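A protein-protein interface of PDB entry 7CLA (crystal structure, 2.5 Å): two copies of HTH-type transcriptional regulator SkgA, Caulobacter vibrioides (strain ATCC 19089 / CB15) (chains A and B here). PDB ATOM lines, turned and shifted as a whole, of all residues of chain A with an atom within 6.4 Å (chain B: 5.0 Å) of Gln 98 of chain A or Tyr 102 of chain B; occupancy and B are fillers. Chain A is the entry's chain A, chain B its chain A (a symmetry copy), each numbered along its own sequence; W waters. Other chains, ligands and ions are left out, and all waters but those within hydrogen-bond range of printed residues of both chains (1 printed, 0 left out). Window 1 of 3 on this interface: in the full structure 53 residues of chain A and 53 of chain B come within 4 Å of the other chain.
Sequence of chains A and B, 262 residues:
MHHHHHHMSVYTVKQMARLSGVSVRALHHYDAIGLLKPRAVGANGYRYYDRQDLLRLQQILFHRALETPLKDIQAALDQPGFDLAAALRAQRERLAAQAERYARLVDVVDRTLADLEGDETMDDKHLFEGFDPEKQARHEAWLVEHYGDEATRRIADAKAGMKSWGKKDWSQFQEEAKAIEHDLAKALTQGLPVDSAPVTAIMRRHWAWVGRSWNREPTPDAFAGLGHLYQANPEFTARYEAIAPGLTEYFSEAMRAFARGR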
ATOM      1  N   ARG A  64     -26.599  26.452  26.418  1.00  0.00           N
ATOM      2  CA  ARG A  64     -27.154  25.269  27.103  1.00  0.00           C
ATOM      3  C   ARG A  64     -26.633  23.980  26.475  1.00  0.00           C
ATOM      4  O   ARG A  64     -26.537  23.012  27.180  1.00  0.00           O
ATOM      5  CB  ARG A  64     -28.670  25.398  27.198  1.00  0.00           C
ATOM      6  CG  ARG A  64     -29.071  26.518  28.140  1.00  0.00           C
ATOM      7  CD  ARG A  64     -30.552  26.549  28.357  1.00  0.00           C
ATOM      8  NE  ARG A  64     -30.953  25.185  28.612  1.00  0.00           N
ATOM      9  CZ  ARG A  64     -31.931  24.564  27.985  1.00  0.00           C
ATOM     10  NH1 ARG A  64     -32.628  25.188  27.055  1.00  0.00           N
ATOM     11  NH2 ARG A  64     -32.214  23.317  28.302  1.00  0.00           N
ATOM     12  N   ALA A  65     -26.355  23.978  25.185  1.00  0.00           N
ATOM     13  CA  ALA A  65     -25.768  22.808  24.537  1.00  0.00           C
ATOM     14  C   ALA A  65     -24.393  22.597  25.152  1.00  0.00           C
ATOM     15  O   ALA A  65     -23.985  21.444  25.269  1.00  0.00           O
ATOM     16  CB  ALA A  65     -25.661  23.020  23.068  1.00  0.00           C
ATOM     17  N   LEU A  66     -23.715  23.693  25.477  1.00  0.00           N
ATOM     18  CA  LEU A  66     -22.341  23.686  26.018  1.00  0.00           C
ATOM     19  C   LEU A  66     -22.354  23.748  27.544  1.00  0.00           C
ATOM     20  O   LEU A  66     -21.324  24.151  28.086  1.00  0.00           O
ATOM     21  CB  LEU A  66     -21.577  24.881  25.447  1.00  0.00           C
ATOM     22  CG  LEU A  66     -21.172  24.703  23.995  1.00  0.00           C
ATOM     23  CD1 LEU A  66     -20.633  25.993  23.441  1.00  0.00           C
ATOM     24  CD2 LEU A  66     -20.185  23.598  23.860  1.00  0.00           C
ATOM     25  N   GLU A  67     -23.489  23.404  28.155  1.00  0.00           N
ATOM     26  CA  GLU A  67     -23.702  23.239  29.622  1.00  0.00           C
ATOM     27  C   GLU A  67     -23.280  24.479  30.422  1.00  0.00           C
ATOM     28  O   GLU A  67     -22.859  24.288  31.546  1.00  0.00           O
ATOM     29  CB  GLU A  67     -22.962  21.982  30.078  1.00  0.00           C
ATOM     30  CG  GLU A  67     -23.802  20.718  29.879  1.00  0.00           C
ATOM     31  CD  GLU A  67     -23.028  19.399  29.800  1.00  0.00           C
ATOM     32  OE1 GLU A  67     -23.707  18.344  29.884  1.00  0.00           O
ATOM     33  OE2 GLU A  67     -21.764  19.405  29.591  1.00  0.00           O
ATOM     34  N   GLU A  93     -16.000  26.335  17.901  1.00  0.00           N
ATOM     35  CA  GLU A  93     -14.757  25.637  18.351  1.00  0.00           C
ATOM     36  C   GLU A  93     -15.080  24.603  19.433  1.00  0.00           C
ATOM     37  O   GLU A  93     -14.603  23.479  19.346  1.00  0.00           O
ATOM     38  CB  GLU A  93     -13.780  26.687  18.869  1.00  0.00           C
ATOM     39  CG  GLU A  93     -12.366  26.505  18.399  1.00  0.00           C
ATOM     40  CD  GLU A  93     -11.370  27.210  19.322  1.00  0.00           C
ATOM     41  OE1 GLU A  93     -11.544  28.446  19.563  1.00  0.00           O
ATOM     42  OE2 GLU A  93     -10.444  26.512  19.847  1.00  0.00           O
ATOM     43  N   ARG A  94     -15.910  24.976  20.378  1.00  0.00           N
ATOM     44  CA  ARG A  94     -16.304  24.144  21.524  1.00  0.00           C
ATOM     45  C   ARG A  94     -17.284  23.059  21.087  1.00  0.00           C
ATOM     46  O   ARG A  94     -17.132  21.895  21.508  1.00  0.00           O
ATOM     47  CB  ARG A  94     -16.894  25.035  22.607  1.00  0.00           C
ATOM     48  CG  ARG A  94     -15.838  25.887  23.297  1.00  0.00           C
ATOM     49  CD  ARG A  94     -16.501  26.745  24.350  1.00  0.00           C
ATOM     50  NE  ARG A  94     -17.103  25.969  25.428  1.00  0.00           N
ATOM     51  CZ  ARG A  94     -17.873  26.523  26.359  1.00  0.00           C
ATOM     52  NH1 ARG A  94     -18.131  27.826  26.283  1.00  0.00           N
ATOM     53  NH2 ARG A  94     -18.417  25.774  27.319  1.00  0.00           N
ATOM     54  N   LEU A  95     -18.227  23.389  20.217  1.00  0.00           N
ATOM     55  CA  LEU A  95     -19.121  22.373  19.609  1.00  0.00           C
ATOM     56  C   LEU A  95     -18.312  21.386  18.757  1.00  0.00           C
ATOM     57  O   LEU A  95     -18.594  20.141  18.827  1.00  0.00           O
ATOM     58  CB  LEU A  95     -20.178  23.075  18.754  1.00  0.00           C
ATOM     59  CG  LEU A  95     -21.120  24.008  19.513  1.00  0.00           C
ATOM     60  CD1 LEU A  95     -21.822  24.955  18.537  1.00  0.00           C
ATOM     61  CD2 LEU A  95     -22.129  23.211  20.315  1.00  0.00           C
ATOM     62  N   ALA A  96     -17.413  21.882  17.922  1.00  0.00           N
ATOM     63  CA  ALA A  96     -16.540  20.993  17.093  1.00  0.00           C
ATOM     64  C   ALA A  96     -15.783  20.050  18.051  1.00  0.00           C
ATOM     65  O   ALA A  96     -15.726  18.822  17.838  1.00  0.00           O
ATOM     66  CB  ALA A  96     -15.610  21.769  16.189  1.00  0.00           C
ATOM     67  N   ALA A  97     -15.242  20.578  19.135  1.00  0.00           N
ATOM     68  CA  ALA A  97     -14.404  19.754  20.033  1.00  0.00           C
ATOM     69  C   ALA A  97     -15.281  18.624  20.620  1.00  0.00           C
ATOM     70  O   ALA A  97     -14.797  17.472  20.667  1.00  0.00           O
ATOM     71  CB  ALA A  97     -13.787  20.641  21.084  1.00  0.00           C
ATOM     72  N   GLN A  98     -16.538  18.918  20.989  1.00  0.00           N
ATOM     73  CA  GLN A  98     -17.509  17.920  21.514  1.00  0.00           C
ATOM     74  C   GLN A  98     -17.795  16.859  20.430  1.00  0.00           C
ATOM     75  O   GLN A  98     -17.740  15.659  20.730  1.00  0.00           O
ATOM     76  CB  GLN A  98     -18.789  18.593  21.999  1.00  0.00           C
ATOM     77  CG  GLN A  98     -18.676  19.245  23.389  1.00  0.00           C
ATOM     78  CD  GLN A  98     -18.064  18.381  24.487  1.00  0.00           C
ATOM     79  OE1 GLN A  98     -18.669  17.420  24.976  1.00  0.00           O
ATOM     80  NE2 GLN A  98     -16.828  18.707  24.878  1.00  0.00           N
ATOM     81  N   ALA A  99     -17.984  17.253  19.188  1.00  0.00           N
ATOM     82  CA  ALA A  99     -18.213  16.314  18.066  1.00  0.00           C
ATOM     83  C   ALA A  99     -17.001  15.368  17.929  1.00  0.00           C
ATOM     84  O   ALA A  99     -17.212  14.189  17.753  1.00  0.00           O
ATOM     85  CB  ALA A  99     -18.486  17.066  16.784  1.00  0.00           C
ATOM     86  N   GLU A 100     -15.787  15.892  18.049  1.00  0.00           N
ATOM     87  CA  GLU A 100     -14.506  15.137  17.930  1.00  0.00           C
ATOM     88  C   GLU A 100     -14.385  14.195  19.139  1.00  0.00           C
ATOM     89  O   GLU A 100     -14.100  13.005  18.934  1.00  0.00           O
ATOM     90  CB  GLU A 100     -13.295  16.075  17.764  1.00  0.00           C
ATOM     91  CG  GLU A 100     -13.120  16.671  16.360  1.00  0.00           C
ATOM     92  CD  GLU A 100     -12.454  18.065  16.330  1.00  0.00           C
ATOM     93  OE1 GLU A 100     -11.681  18.404  17.282  1.00  0.00           O
ATOM     94  OE2 GLU A 100     -12.734  18.872  15.383  1.00  0.00           O
ATOM     95  N   ARG A 101     -14.622  14.681  20.361  1.00  0.00           N
ATOM     96  CA  ARG A 101     -14.658  13.772  21.525  1.00  0.00           C
ATOM     97  C   ARG A 101     -15.600  12.579  21.284  1.00  0.00           C
ATOM     98  O   ARG A 101     -15.250  11.435  21.587  1.00  0.00           O
ATOM     99  CB  ARG A 101     -15.066  14.540  22.774  1.00  0.00           C
ATOM    100  CG  ARG A 101     -14.631  13.827  24.046  1.00  0.00           C
ATOM    101  CD  ARG A 101     -14.431  14.783  25.214  1.00  0.00           C
ATOM    102  NE  ARG A 101     -13.133  15.472  25.351  1.00  0.00           N
ATOM    103  CZ  ARG A 101     -11.916  14.885  25.378  1.00  0.00           C
ATOM    104  NH1 ARG A 101     -11.769  13.579  25.203  1.00  0.00           N
ATOM    105  NH2 ARG A 101     -10.839  15.634  25.562  1.00  0.00           N
ATOM    106  N   TYR A 102     -16.823  12.807  20.809  1.00  0.00           N
ATOM    107  CA  TYR A 102     -17.822  11.716  20.698  1.00  0.00           C
ATOM    108  C   TYR A 102     -17.380  10.768  19.592  1.00  0.00           C
ATOM    109  O   TYR A 102     -17.613   9.524  19.704  1.00  0.00           O
ATOM    110  CB  TYR A 102     -19.239  12.296  20.606  1.00  0.00           C
ATOM    111  CG  TYR A 102     -19.760  12.649  21.980  1.00  0.00           C
ATOM    112  CD1 TYR A 102     -20.082  11.635  22.872  1.00  0.00           C
ATOM    113  CD2 TYR A 102     -19.843  13.955  22.425  1.00  0.00           C
ATOM    114  CE1 TYR A 102     -20.425  11.892  24.175  1.00  0.00           C
ATOM    115  CE2 TYR A 102     -20.222  14.237  23.723  1.00  0.00           C
ATOM    116  CZ  TYR A 102     -20.485  13.201  24.599  1.00  0.00           C
ATOM    117  OH  TYR A 102     -20.846  13.454  25.887  1.00  0.00           O
ATOM    118  N   ALA A 103     -16.721  11.304  18.569  1.00  0.00           N
ATOM    119  CA  ALA A 103     -16.303  10.512  17.398  1.00  0.00           C
ATOM    120  C   ALA A 103     -15.103   9.620  17.810  1.00  0.00           C
ATOM    121  O   ALA A 103     -14.996   8.468  17.285  1.00  0.00           O
ATOM    122  CB  ALA A 103     -16.008  11.426  16.234  1.00  0.00           C
ATOM    123  N   ASP A 132     -12.950  12.316  28.616  1.00  0.00           N
ATOM    124  CA  ASP A 132     -12.834  13.760  28.958  1.00  0.00           C
ATOM    125  C   ASP A 132     -12.247  13.876  30.366  1.00  0.00           C
ATOM    126  O   ASP A 132     -12.860  13.477  31.346  1.00  0.00           O
ATOM    127  CB  ASP A 132     -14.207  14.435  28.809  1.00  0.00           C
ATOM    128  CG  ASP A 132     -14.241  15.958  28.810  1.00  0.00           C
ATOM    129  OD1 ASP A 132     -13.349  16.600  29.479  1.00  0.00           O
ATOM    130  OD2 ASP A 132     -15.209  16.486  28.202  1.00  0.00           O
ATOM    131  N   LYS A 135     -14.463  16.132  32.777  1.00  0.00           N
ATOM    132  CA  LYS A 135     -15.658  15.431  33.308  1.00  0.00           C
ATOM    133  C   LYS A 135     -15.272  14.451  34.421  1.00  0.00           C
ATOM    134  O   LYS A 135     -16.147  14.113  35.229  1.00  0.00           O
ATOM    135  CB  LYS A 135     -16.367  14.674  32.189  1.00  0.00           C
ATOM    136  CG  LYS A 135     -17.058  15.571  31.184  1.00  0.00           C
ATOM    137  CD  LYS A 135     -18.384  15.050  30.709  1.00  0.00           C
ATOM    138  CE  LYS A 135     -19.270  16.181  30.243  1.00  0.00           C
ATOM    139  NZ  LYS A 135     -18.908  17.436  30.934  1.00  0.00           N
ATOM    140  N   GLN B  98     -24.523  11.529  19.577  1.00  0.00           N
ATOM    141  CA  GLN B  98     -23.959  12.743  20.227  1.00  0.00           C
ATOM    142  C   GLN B  98     -22.964  13.427  19.267  1.00  0.00           C
ATOM    143  O   GLN B  98     -23.054  14.646  19.071  1.00  0.00           O
ATOM    144  CB  GLN B  98     -23.314  12.406  21.567  1.00  0.00           C
ATOM    145  CG  GLN B  98     -24.311  12.225  22.725  1.00  0.00           C
ATOM    146  CD  GLN B  98     -25.360  13.320  22.885  1.00  0.00           C
ATOM    147  OE1 GLN B  98     -25.070  14.447  23.299  1.00  0.00           O
ATOM    148  NE2 GLN B  98     -26.610  13.001  22.532  1.00  0.00           N
ATOM    149  N   ALA B  99     -22.110  12.682  18.597  1.00  0.00           N
ATOM    150  CA  ALA B  99     -21.150  13.232  17.614  1.00  0.00           C
ATOM    151  C   ALA B  99     -21.922  13.945  16.482  1.00  0.00           C
ATOM    152  O   ALA B  99     -21.517  15.022  16.104  1.00  0.00           O
ATOM    153  CB  ALA B  99     -20.246  12.145  17.079  1.00  0.00           C
ATOM    154  N   GLU B 100     -23.012  13.355  16.006  1.00  0.00           N
ATOM    155  CA  GLU B 100     -23.870  13.886  14.907  1.00  0.00           C
ATOM    156  C   GLU B 100     -24.589  15.145  15.420  1.00  0.00           C
ATOM    157  O   GLU B 100     -24.560  16.168  14.718  1.00  0.00           O
ATOM    158  CB  GLU B 100     -24.832  12.816  14.357  1.00  0.00           C
ATOM    159  CG  GLU B 100     -24.191  11.787  13.413  1.00  0.00           C
ATOM    160  CD  GLU B 100     -24.855  10.392  13.436  1.00  0.00           C
ATOM    161  OE1 GLU B 100     -26.076  10.291  13.776  1.00  0.00           O
ATOM    162  OE2 GLU B 100     -24.153   9.361  13.168  1.00  0.00           O
ATOM    163  N   ARG B 101     -25.190  15.104  16.612  1.00  0.00           N
ATOM    164  CA  ARG B 101     -25.761  16.335  17.196  1.00  0.00           C
ATOM    165  C   ARG B 101     -24.739  17.485  17.206  1.00  0.00           C
ATOM    166  O   ARG B 101     -25.072  18.619  16.851  1.00  0.00           O
ATOM    167  CB  ARG B 101     -26.276  16.056  18.601  1.00  0.00           C
ATOM    168  CG  ARG B 101     -27.306  17.085  19.042  1.00  0.00           C
ATOM    169  CD  ARG B 101     -28.273  16.535  20.082  1.00  0.00           C
ATOM    170  NE  ARG B 101     -29.458  15.787  19.621  1.00  0.00           N
ATOM    171  CZ  ARG B 101     -30.372  16.212  18.722  1.00  0.00           C
ATOM    172  NH1 ARG B 101     -30.238  17.370  18.088  1.00  0.00           N
ATOM    173  NH2 ARG B 101     -31.417  15.447  18.447  1.00  0.00           N
ATOM    174  N   TYR B 102     -23.512  17.255  17.666  1.00  0.00           N
ATOM    175  CA  TYR B 102     -22.533  18.357  17.838  1.00  0.00           C
ATOM    176  C   TYR B 102     -22.112  18.847  16.459  1.00  0.00           C
ATOM    177  O   TYR B 102     -21.858  20.080  16.286  1.00  0.00           O
ATOM    178  CB  TYR B 102     -21.422  17.938  18.809  1.00  0.00           C
ATOM    179  CG  TYR B 102     -21.875  18.103  20.240  1.00  0.00           C
ATOM    180  CD1 TYR B 102     -22.045  19.377  20.763  1.00  0.00           C
ATOM    181  CD2 TYR B 102     -22.223  17.024  21.033  1.00  0.00           C
ATOM    182  CE1 TYR B 102     -22.586  19.589  22.007  1.00  0.00           C
ATOM    183  CE2 TYR B 102     -22.735  17.215  22.301  1.00  0.00           C
ATOM    184  CZ  TYR B 102     -22.938  18.499  22.770  1.00  0.00           C
ATOM    185  OH  TYR B 102     -23.456  18.712  24.011  1.00  0.00           O
ATOM    186  N   ALA B 103     -22.078  17.944  15.485  1.00  0.00           N
ATOM    187  CA  ALA B 103     -21.615  18.269  14.123  1.00  0.00           C
ATOM    188  C   ALA B 103     -22.714  19.106  13.418  1.00  0.00           C
ATOM    189  O   ALA B 103     -22.355  20.011  12.602  1.00  0.00           O
ATOM    190  CB  ALA B 103     -21.250  17.004  13.385  1.00  0.00           C
ATOM    191  N   ARG B 104     -23.980  18.802  13.708  1.00  0.00           N
ATOM    192  CA  ARG B 104     -25.183  19.520  13.219  1.00  0.00           C
ATOM    193  C   ARG B 104     -25.189  20.925  13.818  1.00  0.00           C
ATOM    194  O   ARG B 104     -25.457  21.859  13.095  1.00  0.00           O
ATOM    195  CB  ARG B 104     -26.497  18.836  13.635  1.00  0.00           C
ATOM    196  CG  ARG B 104     -27.156  17.939  12.597  1.00  0.00           C
ATOM    197  CD  ARG B 104     -28.501  17.435  13.126  1.00  0.00           C
ATOM    198  NE  ARG B 104     -29.674  18.134  12.565  1.00  0.00           N
ATOM    199  CZ  ARG B 104     -30.924  18.157  13.091  1.00  0.00           C
ATOM    200  NH1 ARG B 104     -31.898  18.793  12.450  1.00  0.00           N
ATOM    201  NH2 ARG B 104     -31.189  17.594  14.264  1.00  0.00           N
ATOM    202  N   LEU B 105     -24.901  21.063  15.107  1.00  0.00           N
ATOM    203  CA  LEU B 105     -24.836  22.396  15.768  1.00  0.00           C
ATOM    204  C   LEU B 105     -23.702  23.239  15.178  1.00  0.00           C
ATOM    205  O   LEU B 105     -23.906  24.427  14.979  1.00  0.00           O
ATOM    206  CB  LEU B 105     -24.733  22.193  17.281  1.00  0.00           C
ATOM    207  CG  LEU B 105     -26.012  21.641  17.915  1.00  0.00           C
ATOM    208  CD1 LEU B 105     -25.818  21.324  19.350  1.00  0.00           C
ATOM    209  CD2 LEU B 105     -27.137  22.617  17.767  1.00  0.00           C
ATOM    210  N   VAL B 106     -22.592  22.655  14.771  1.00  0.00           N
ATOM    211  CA  VAL B 106     -21.528  23.441  14.061  1.00  0.00           C
ATOM    212  C   VAL B 106     -22.111  23.924  12.726  1.00  0.00           C
ATOM    213  O   VAL B 106     -21.827  25.035  12.294  1.00  0.00           O
ATOM    214  CB  VAL B 106     -20.273  22.572  13.839  1.00  0.00           C
ATOM    215  CG1 VAL B 106     -19.279  23.172  12.869  1.00  0.00           C
ATOM    216  CG2 VAL B 106     -19.598  22.191  15.142  1.00  0.00           C
HETATM  217  O   HOH W   1     -25.986  19.801  25.798  1.00  0.00           O
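O of Ala 65 of chain A sits at hydrogen-bond distance from OH of Tyr 102 of chain B (3.1 Å).
Among the printed residues, merely in contact across the chains: Tyr 102 of chain A with Ala 99 of chain B, Ala 99 of chain A with Tyr 102 of chain B, Ala 96 of chain A with Val 106 of chain B, Tyr 102 of chain A with Gln 98 of chain B, Gln 98 of chain A with Tyr 102 of chain B, Leu 95 of chain A with Tyr 102 of chain B, Ala 99 of chain A with Ala 99 of chain B, Leu 95 of chain A with Val 106 of chain B, Ala 103 of chain A with Ala 99 of chain B and Ala 99 of chain A with Ala 103 of chain B.
Of the printed residues of chain B, Gln 98 of chain A touches Tyr 102 (3.6 Å). Of chain A, only Ala 65 (3.1 Å), Leu 95 (3.6 Å), Gln 98 (3.6 Å) and Ala 99 (3.5 Å) come within 4 Å of Tyr 102 of chain B. Printed residues of chain A within 4 Å of Ala 99 of chain B: Ala 99, Tyr 102 and Ala 103. Of the printed residues of chain B, Leu 95 of chain A touches Tyr 102 and Val 106. Of the printed residues of chain A, Gln 98 of chain B touches Tyr 102 (3.6 Å). The nearest printed residue of chain B that does not touch Gln 98 of chain A is Ala 99 of chain B (5.2 Å). The nearest printed residue of chain B that does not touch Ala 96 of chain A is Tyr 102 of chain B (5.1 Å).
Of the 9 printed residues of chain B, 5 touch a printed residue of chain A. Hydrophobic or aromatic side chains of chain A within 4 Å of the printed part of chain B: Leu 95, Ala 99 and Tyr 102.
Gln 98 of chain A touches Tyr 102 of chain B, and with the chains exchanged Tyr 102 of chain A touches Gln 98 of chain B. Ala 99 of chain B touches its own counterpart, Ala 99 of chain A. Ala 99 of chain A touches Tyr 102 of chain B, and with the chains exchanged Tyr 102 of chain A touches Ala 99 of chain B. Ala 99 of chain A touches Ala 103 of chain B, and with the chains exchanged Ala 103 of chain A touches Ala 99 of chain B. Positions printed for both chains: 98, 99, 100, 101, 102 and 103.
Water W1 bridges O of Ala 65 of chain A (2.6 Å) and OH of Tyr 102 of chain B (3.3 Å).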
